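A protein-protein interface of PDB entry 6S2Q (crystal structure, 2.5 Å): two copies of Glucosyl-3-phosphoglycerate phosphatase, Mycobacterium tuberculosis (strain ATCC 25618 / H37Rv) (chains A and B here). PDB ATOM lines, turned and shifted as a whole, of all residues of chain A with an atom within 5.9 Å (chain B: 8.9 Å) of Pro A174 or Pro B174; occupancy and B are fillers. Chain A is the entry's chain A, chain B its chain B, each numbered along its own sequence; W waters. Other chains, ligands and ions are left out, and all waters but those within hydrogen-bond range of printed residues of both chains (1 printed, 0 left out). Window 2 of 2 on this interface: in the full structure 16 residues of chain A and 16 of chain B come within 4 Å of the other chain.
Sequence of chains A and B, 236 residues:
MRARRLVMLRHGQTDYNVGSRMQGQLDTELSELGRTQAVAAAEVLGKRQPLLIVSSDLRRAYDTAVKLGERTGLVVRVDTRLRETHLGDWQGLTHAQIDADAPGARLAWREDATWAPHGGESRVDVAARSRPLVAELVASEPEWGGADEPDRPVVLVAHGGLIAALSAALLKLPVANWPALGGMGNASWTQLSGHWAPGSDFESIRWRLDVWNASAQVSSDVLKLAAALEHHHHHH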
ATOM      1  N   LYS A 172     -20.475   9.876 -18.741  1.00  0.00           N
ATOM      2  CA  LYS A 172     -19.827   9.881 -17.427  1.00  0.00           C
ATOM      3  C   LYS A 172     -18.728   8.833 -17.350  1.00  0.00           C
ATOM      4  O   LYS A 172     -18.525   8.194 -16.323  1.00  0.00           O
ATOM      5  CB  LYS A 172     -20.838   9.696 -16.301  1.00  0.00           C
ATOM      6  CG  LYS A 172     -21.760  10.889 -16.170  1.00  0.00           C
ATOM      7  CD  LYS A 172     -22.745  10.721 -15.029  1.00  0.00           C
ATOM      8  CE  LYS A 172     -23.769  11.864 -15.010  1.00  0.00           C
ATOM      9  NZ  LYS A 172     -25.172  11.386 -15.208  1.00  0.00           N
ATOM     10  N   LEU A 173     -18.025   8.651 -18.451  1.00  0.00           N
ATOM     11  CA  LEU A 173     -16.819   7.849 -18.423  1.00  0.00           C
ATOM     12  C   LEU A 173     -15.750   8.541 -17.587  1.00  0.00           C
ATOM     13  O   LEU A 173     -15.624   9.770 -17.635  1.00  0.00           O
ATOM     14  CB  LEU A 173     -16.254   7.647 -19.822  1.00  0.00           C
ATOM     15  CG  LEU A 173     -16.962   6.935 -20.950  1.00  0.00           C
ATOM     16  CD1 LEU A 173     -15.974   6.903 -22.117  1.00  0.00           C
ATOM     17  CD2 LEU A 173     -17.326   5.533 -20.499  1.00  0.00           C
ATOM     18  N   PRO A 174     -14.945   7.788 -16.842  1.00  0.00           N
ATOM     19  CA  PRO A 174     -13.759   8.400 -16.237  1.00  0.00           C
ATOM     20  C   PRO A 174     -12.889   9.004 -17.331  1.00  0.00           C
ATOM     21  O   PRO A 174     -12.766   8.455 -18.428  1.00  0.00           O
ATOM     22  CB  PRO A 174     -13.070   7.225 -15.527  1.00  0.00           C
ATOM     23  CG  PRO A 174     -14.132   6.161 -15.418  1.00  0.00           C
ATOM     24  CD  PRO A 174     -15.023   6.335 -16.591  1.00  0.00           C
ATOM     25  N   VAL A 175     -12.290  10.154 -17.022  1.00  0.00           N
ATOM     26  CA  VAL A 175     -11.473  10.867 -18.004  1.00  0.00           C
ATOM     27  C   VAL A 175     -10.348   9.982 -18.565  1.00  0.00           C
ATOM     28  O   VAL A 175      -9.940  10.131 -19.732  1.00  0.00           O
ATOM     29  CB  VAL A 175     -10.942  12.166 -17.362  1.00  0.00           C
ATOM     30  CG1 VAL A 175      -9.911  12.838 -18.253  1.00  0.00           C
ATOM     31  CG2 VAL A 175     -12.115  13.115 -17.049  1.00  0.00           C
ATOM     32  N   ALA A 176      -9.826   9.057 -17.753  1.00  0.00           N
ATOM     33  CA  ALA A 176      -8.774   8.163 -18.220  1.00  0.00           C
ATOM     34  C   ALA A 176      -9.232   7.288 -19.380  1.00  0.00           C
ATOM     35  O   ALA A 176      -8.398   6.844 -20.175  1.00  0.00           O
ATOM     36  CB  ALA A 176      -8.286   7.283 -17.064  1.00  0.00           C
ATOM     37  N   ASN A 177     -10.533   7.073 -19.540  1.00  0.00           N
ATOM     38  CA  ASN A 177     -11.014   6.192 -20.597  1.00  0.00           C
ATOM     39  C   ASN A 177     -11.556   6.943 -21.806  1.00  0.00           C
ATOM     40  O   ASN A 177     -11.978   6.303 -22.777  1.00  0.00           O
ATOM     41  CB  ASN A 177     -12.089   5.257 -20.060  1.00  0.00           C
ATOM     42  CG  ASN A 177     -11.602   4.466 -18.907  1.00  0.00           C
ATOM     43  OD1 ASN A 177     -11.870   4.809 -17.758  1.00  0.00           O
ATOM     44  ND2 ASN A 177     -10.797   3.449 -19.187  1.00  0.00           N
ATOM     45  N   TRP A 178     -11.588   8.273 -21.762  1.00  0.00           N
ATOM     46  CA  TRP A 178     -12.051   9.012 -22.930  1.00  0.00           C
ATOM     47  C   TRP A 178     -11.272   8.672 -24.199  1.00  0.00           C
ATOM     48  O   TRP A 178     -11.892   8.629 -25.276  1.00  0.00           O
ATOM     49  CB  TRP A 178     -11.991  10.515 -22.659  1.00  0.00           C
ATOM     50  CG  TRP A 178     -12.963  11.005 -21.656  1.00  0.00           C
ATOM     51  CD1 TRP A 178     -13.588  10.282 -20.695  1.00  0.00           C
ATOM     52  CD2 TRP A 178     -13.432  12.350 -21.518  1.00  0.00           C
ATOM     53  NE1 TRP A 178     -14.417  11.093 -19.954  1.00  0.00           N
ATOM     54  CE2 TRP A 178     -14.340  12.367 -20.448  1.00  0.00           C
ATOM     55  CE3 TRP A 178     -13.162  13.544 -22.193  1.00  0.00           C
ATOM     56  CZ2 TRP A 178     -14.975  13.528 -20.037  1.00  0.00           C
ATOM     57  CZ3 TRP A 178     -13.788  14.682 -21.793  1.00  0.00           C
ATOM     58  CH2 TRP A 178     -14.685  14.677 -20.729  1.00  0.00           C
ATOM     59  N   ALA B 113     -22.976  -4.787 -14.384  1.00  0.00           N
ATOM     60  CA  ALA B 113     -22.321  -5.833 -15.165  1.00  0.00           C
ATOM     61  C   ALA B 113     -21.868  -6.992 -14.307  1.00  0.00           C
ATOM     62  O   ALA B 113     -21.477  -8.030 -14.855  1.00  0.00           O
ATOM     63  CB  ALA B 113     -21.115  -5.274 -15.918  1.00  0.00           C
ATOM     64  N   THR B 114     -21.946  -6.851 -12.987  1.00  0.00           N
ATOM     65  CA  THR B 114     -21.554  -7.922 -12.094  1.00  0.00           C
ATOM     66  C   THR B 114     -22.719  -8.816 -11.714  1.00  0.00           C
ATOM     67  O   THR B 114     -22.487  -9.931 -11.229  1.00  0.00           O
ATOM     68  CB  THR B 114     -20.932  -7.366 -10.800  1.00  0.00           C
ATOM     69  OG1 THR B 114     -21.868  -6.495 -10.157  1.00  0.00           O
ATOM     70  CG2 THR B 114     -19.633  -6.635 -11.052  1.00  0.00           C
ATOM     71  N   VAL B 124     -19.595  -9.557 -16.589  1.00  0.00           N
ATOM     72  CA  VAL B 124     -18.208  -9.847 -16.268  1.00  0.00           C
ATOM     73  C   VAL B 124     -17.892 -11.311 -16.562  1.00  0.00           C
ATOM     74  O   VAL B 124     -16.820 -11.635 -17.091  1.00  0.00           O
ATOM     75  CB  VAL B 124     -17.917  -9.446 -14.805  1.00  0.00           C
ATOM     76  CG1 VAL B 124     -16.563  -9.936 -14.362  1.00  0.00           C
ATOM     77  CG2 VAL B 124     -17.958  -7.917 -14.658  1.00  0.00           C
ATOM     78  N   ALA B 168     -16.218  -3.872 -23.933  1.00  0.00           N
ATOM     79  CA  ALA B 168     -15.926  -3.145 -22.702  1.00  0.00           C
ATOM     80  C   ALA B 168     -14.700  -3.716 -22.007  1.00  0.00           C
ATOM     81  O   ALA B 168     -13.877  -2.966 -21.472  1.00  0.00           O
ATOM     82  CB  ALA B 168     -17.136  -3.170 -21.772  1.00  0.00           C
ATOM     83  N   ALA B 169     -14.566  -5.044 -21.982  1.00  0.00           N
ATOM     84  CA  ALA B 169     -13.390  -5.620 -21.343  1.00  0.00           C
ATOM     85  C   ALA B 169     -12.126  -5.284 -22.126  1.00  0.00           C
ATOM     86  O   ALA B 169     -11.129  -4.854 -21.546  1.00  0.00           O
ATOM     87  CB  ALA B 169     -13.549  -7.135 -21.164  1.00  0.00           C
ATOM     88  N   LEU B 171     -11.655  -2.764 -24.100  1.00  0.00           N
ATOM     89  CA  LEU B 171     -11.467  -1.330 -23.902  1.00  0.00           C
ATOM     90  C   LEU B 171     -11.017  -0.995 -22.497  1.00  0.00           C
ATOM     91  O   LEU B 171     -10.806   0.184 -22.204  1.00  0.00           O
ATOM     92  CB  LEU B 171     -12.755  -0.568 -24.211  1.00  0.00           C
ATOM     93  CG  LEU B 171     -13.201  -0.671 -25.667  1.00  0.00           C
ATOM     94  CD1 LEU B 171     -14.643  -0.209 -25.885  1.00  0.00           C
ATOM     95  CD2 LEU B 171     -12.257   0.150 -26.520  1.00  0.00           C
ATOM     96  N   LYS B 172     -10.951  -1.984 -21.616  1.00  0.00           N
ATOM     97  CA  LYS B 172     -10.511  -1.793 -20.237  1.00  0.00           C
ATOM     98  C   LYS B 172     -11.304  -0.689 -19.553  1.00  0.00           C
ATOM     99  O   LYS B 172     -10.767   0.073 -18.745  1.00  0.00           O
ATOM    100  CB  LYS B 172      -9.016  -1.493 -20.198  1.00  0.00           C
ATOM    101  CG  LYS B 172      -8.197  -2.642 -20.709  1.00  0.00           C
ATOM    102  CD  LYS B 172      -6.732  -2.336 -20.716  1.00  0.00           C
ATOM    103  CE  LYS B 172      -6.034  -3.437 -21.474  1.00  0.00           C
ATOM    104  NZ  LYS B 172      -4.568  -3.510 -21.253  1.00  0.00           N
ATOM    105  N   LEU B 173     -12.577  -0.575 -19.883  1.00  0.00           N
ATOM    106  CA  LEU B 173     -13.458   0.311 -19.144  1.00  0.00           C
ATOM    107  C   LEU B 173     -13.641  -0.212 -17.717  1.00  0.00           C
ATOM    108  O   LEU B 173     -13.630  -1.426 -17.490  1.00  0.00           O
ATOM    109  CB  LEU B 173     -14.804   0.412 -19.856  1.00  0.00           C
ATOM    110  CG  LEU B 173     -14.730   0.958 -21.282  1.00  0.00           C
ATOM    111  CD1 LEU B 173     -16.107   1.102 -21.846  1.00  0.00           C
ATOM    112  CD2 LEU B 173     -14.039   2.313 -21.288  1.00  0.00           C
ATOM    113  N   PRO B 174     -13.759   0.667 -16.722  1.00  0.00           N
ATOM    114  CA  PRO B 174     -14.127   0.184 -15.390  1.00  0.00           C
ATOM    115  C   PRO B 174     -15.456  -0.539 -15.463  1.00  0.00           C
ATOM    116  O   PRO B 174     -16.361  -0.128 -16.188  1.00  0.00           O
ATOM    117  CB  PRO B 174     -14.218   1.466 -14.552  1.00  0.00           C
ATOM    118  CG  PRO B 174     -13.478   2.505 -15.318  1.00  0.00           C
ATOM    119  CD  PRO B 174     -13.655   2.136 -16.764  1.00  0.00           C
ATOM    120  N   VAL B 175     -15.567  -1.621 -14.685  1.00  0.00           N
ATOM    121  CA  VAL B 175     -16.783  -2.437 -14.690  1.00  0.00           C
ATOM    122  C   VAL B 175     -18.019  -1.589 -14.390  1.00  0.00           C
ATOM    123  O   VAL B 175     -19.110  -1.855 -14.918  1.00  0.00           O
ATOM    124  CB  VAL B 175     -16.637  -3.609 -13.696  1.00  0.00           C
ATOM    125  CG1 VAL B 175     -17.970  -4.306 -13.498  1.00  0.00           C
ATOM    126  CG2 VAL B 175     -15.571  -4.599 -14.174  1.00  0.00           C
ATOM    127  N   ALA B 176     -17.873  -0.553 -13.558  1.00  0.00           N
ATOM    128  CA  ALA B 176     -18.988   0.341 -13.276  1.00  0.00           C
ATOM    129  C   ALA B 176     -19.474   1.040 -14.532  1.00  0.00           C
ATOM    130  O   ALA B 176     -20.598   1.554 -14.547  1.00  0.00           O
ATOM    131  CB  ALA B 176     -18.582   1.385 -12.241  1.00  0.00           C
ATOM    132  N   ASN B 177     -18.649   1.090 -15.581  1.00  0.00           N
ATOM    133  CA  ASN B 177     -18.987   1.831 -16.786  1.00  0.00           C
ATOM    134  C   ASN B 177     -19.455   0.965 -17.946  1.00  0.00           C
ATOM    135  O   ASN B 177     -19.938   1.513 -18.937  1.00  0.00           O
ATOM    136  CB  ASN B 177     -17.781   2.675 -17.212  1.00  0.00           C
ATOM    137  CG  ASN B 177     -17.404   3.704 -16.160  1.00  0.00           C
ATOM    138  OD1 ASN B 177     -16.553   3.450 -15.305  1.00  0.00           O
ATOM    139  ND2 ASN B 177     -18.020   4.880 -16.231  1.00  0.00           N
ATOM    140  N   TRP B 178     -19.408  -0.351 -17.821  1.00  0.00           N
ATOM    141  CA  TRP B 178     -19.883  -1.267 -18.856  1.00  0.00           C
ATOM    142  C   TRP B 178     -21.322  -1.027 -19.320  1.00  0.00           C
ATOM    143  O   TRP B 178     -21.617  -1.281 -20.497  1.00  0.00           O
ATOM    144  CB  TRP B 178     -19.749  -2.716 -18.371  1.00  0.00           C
ATOM    145  CG  TRP B 178     -18.329  -3.193 -18.304  1.00  0.00           C
ATOM    146  CD1 TRP B 178     -17.213  -2.423 -18.233  1.00  0.00           C
ATOM    147  CD2 TRP B 178     -17.875  -4.550 -18.353  1.00  0.00           C
ATOM    148  NE1 TRP B 178     -16.091  -3.211 -18.205  1.00  0.00           N
ATOM    149  CE2 TRP B 178     -16.470  -4.522 -18.283  1.00  0.00           C
ATOM    150  CE3 TRP B 178     -18.523  -5.792 -18.429  1.00  0.00           C
ATOM    151  CZ2 TRP B 178     -15.698  -5.682 -18.291  1.00  0.00           C
ATOM    152  CZ3 TRP B 178     -17.755  -6.943 -18.432  1.00  0.00           C
ATOM    153  CH2 TRP B 178     -16.360  -6.880 -18.367  1.00  0.00           C
ATOM    154  N   PRO B 179     -22.257  -0.582 -18.465  1.00  0.00           N
ATOM    155  CA  PRO B 179     -23.618  -0.300 -18.968  1.00  0.00           C
ATOM    156  C   PRO B 179     -23.684   0.796 -20.020  1.00  0.00           C
ATOM    157  O   PRO B 179     -24.737   0.938 -20.661  1.00  0.00           O
ATOM    158  CB  PRO B 179     -24.380   0.122 -17.702  1.00  0.00           C
ATOM    159  CG  PRO B 179     -23.665  -0.545 -16.604  1.00  0.00           C
ATOM    160  CD  PRO B 179     -22.219  -0.538 -16.985  1.00  0.00           C
ATOM    161  N   ALA B 180     -22.602   1.551 -20.241  1.00  0.00           N
ATOM    162  CA  ALA B 180     -22.636   2.611 -21.238  1.00  0.00           C
ATOM    163  C   ALA B 180     -22.807   2.061 -22.645  1.00  0.00           C
ATOM    164  O   ALA B 180     -23.419   2.723 -23.497  1.00  0.00           O
ATOM    165  CB  ALA B 180     -21.369   3.451 -21.152  1.00  0.00           C
HETATM  166  O   HOH W   1      -9.734   3.431 -22.093  1.00  0.00           O
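Water W1 bridges ND2 of Asn A177 (3.1 Å) and O of Leu B171 (3.4 Å).
Lys A172 touches Asn B177, and with the chains exchanged Asn A177 touches Lys B172. Leu A173 touches Asn B177, and with the chains exchanged Asn A177 touches Leu B173. Pro A174 touches its own counterpart, Pro B174. Pro A174 touches Asn B177, and with the chains exchanged Asn A177 touches Pro B174. Of the 7 pairs that touch across the chains among the printed residues, 7 have their exchanged pair printed and touching as well.
The backbone carbonyl oxygen (O) of Lys B172 lies within hydrogen-bond range of the side-chain amide nitrogen (ND2) of Asn A177 (3.4 Å). The side-chain amide nitrogen of Asn B177 lies within hydrogen-bond range of the backbone carbonyl oxygen of Lys A172 (3.4 Å).
Among the printed residues, merely in contact across the chains: Leu A173 with Asn B177 (3.9 Å), Pro A174 with Pro B174 (3.7 Å), Pro A174 with Asn B177 (3.4 Å), Asn A177 with Leu B173 (3.7 Å) and Asn A177 with Pro B174 (3.4 Å).
Pro A174 touches two residues of chain B. Of chain A, only Pro A174 (3.7 Å) and Asn A177 (3.4 Å) come within 4 Å of Pro B174. Of the printed residues of chain B, Lys A172 touches Asn B177 (3.4 Å). Of the printed residues of chain A, Lys B172 touches Asn A177. Of the printed residues of chain A, Asn B177 touches Lys A172 (3.4 Å), Leu A173 (3.9 Å) and Pro A174 (3.4 Å). The nearest residue of chain B that does not touch Pro A174 is Leu B173 (6.3 Å). The nearest printed residue of chain A that does not touch Pro B174 is Leu A173 (6.2 Å). The nearest printed residue of chain A that does not touch Asn B177 is Asn A177 (5.5 Å).
The backbone carbonyl oxygen (O) of Ala B168 is in hydrogen-bond range of the backbone NH (N) of Leu B173 (3.2 Å). The backbone carbonyl oxygen (O) of Leu A173 sits at hydrogen-bond distance from the indole nitrogen (NE1) of Trp A178 (2.9 Å). The indole nitrogen of Trp B178 lies within hydrogen-bond range of the backbone carbonyl oxygen of Leu B173 (3.1 Å). The backbone carbonyl oxygen of Pro A174 sits close to the indole nitrogen of Trp A178 (3.5 Å).
Of the 15 printed residues of chain B, 4 touch a printed residue of chain A. Of the 7 printed residues of chain A, 4 touch a printed residue of chain B. Along chain A the printed residues that touch a printed residue of chain B span positions 172 to 177. Among the printed residues, 7 pairs touch across the chains.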
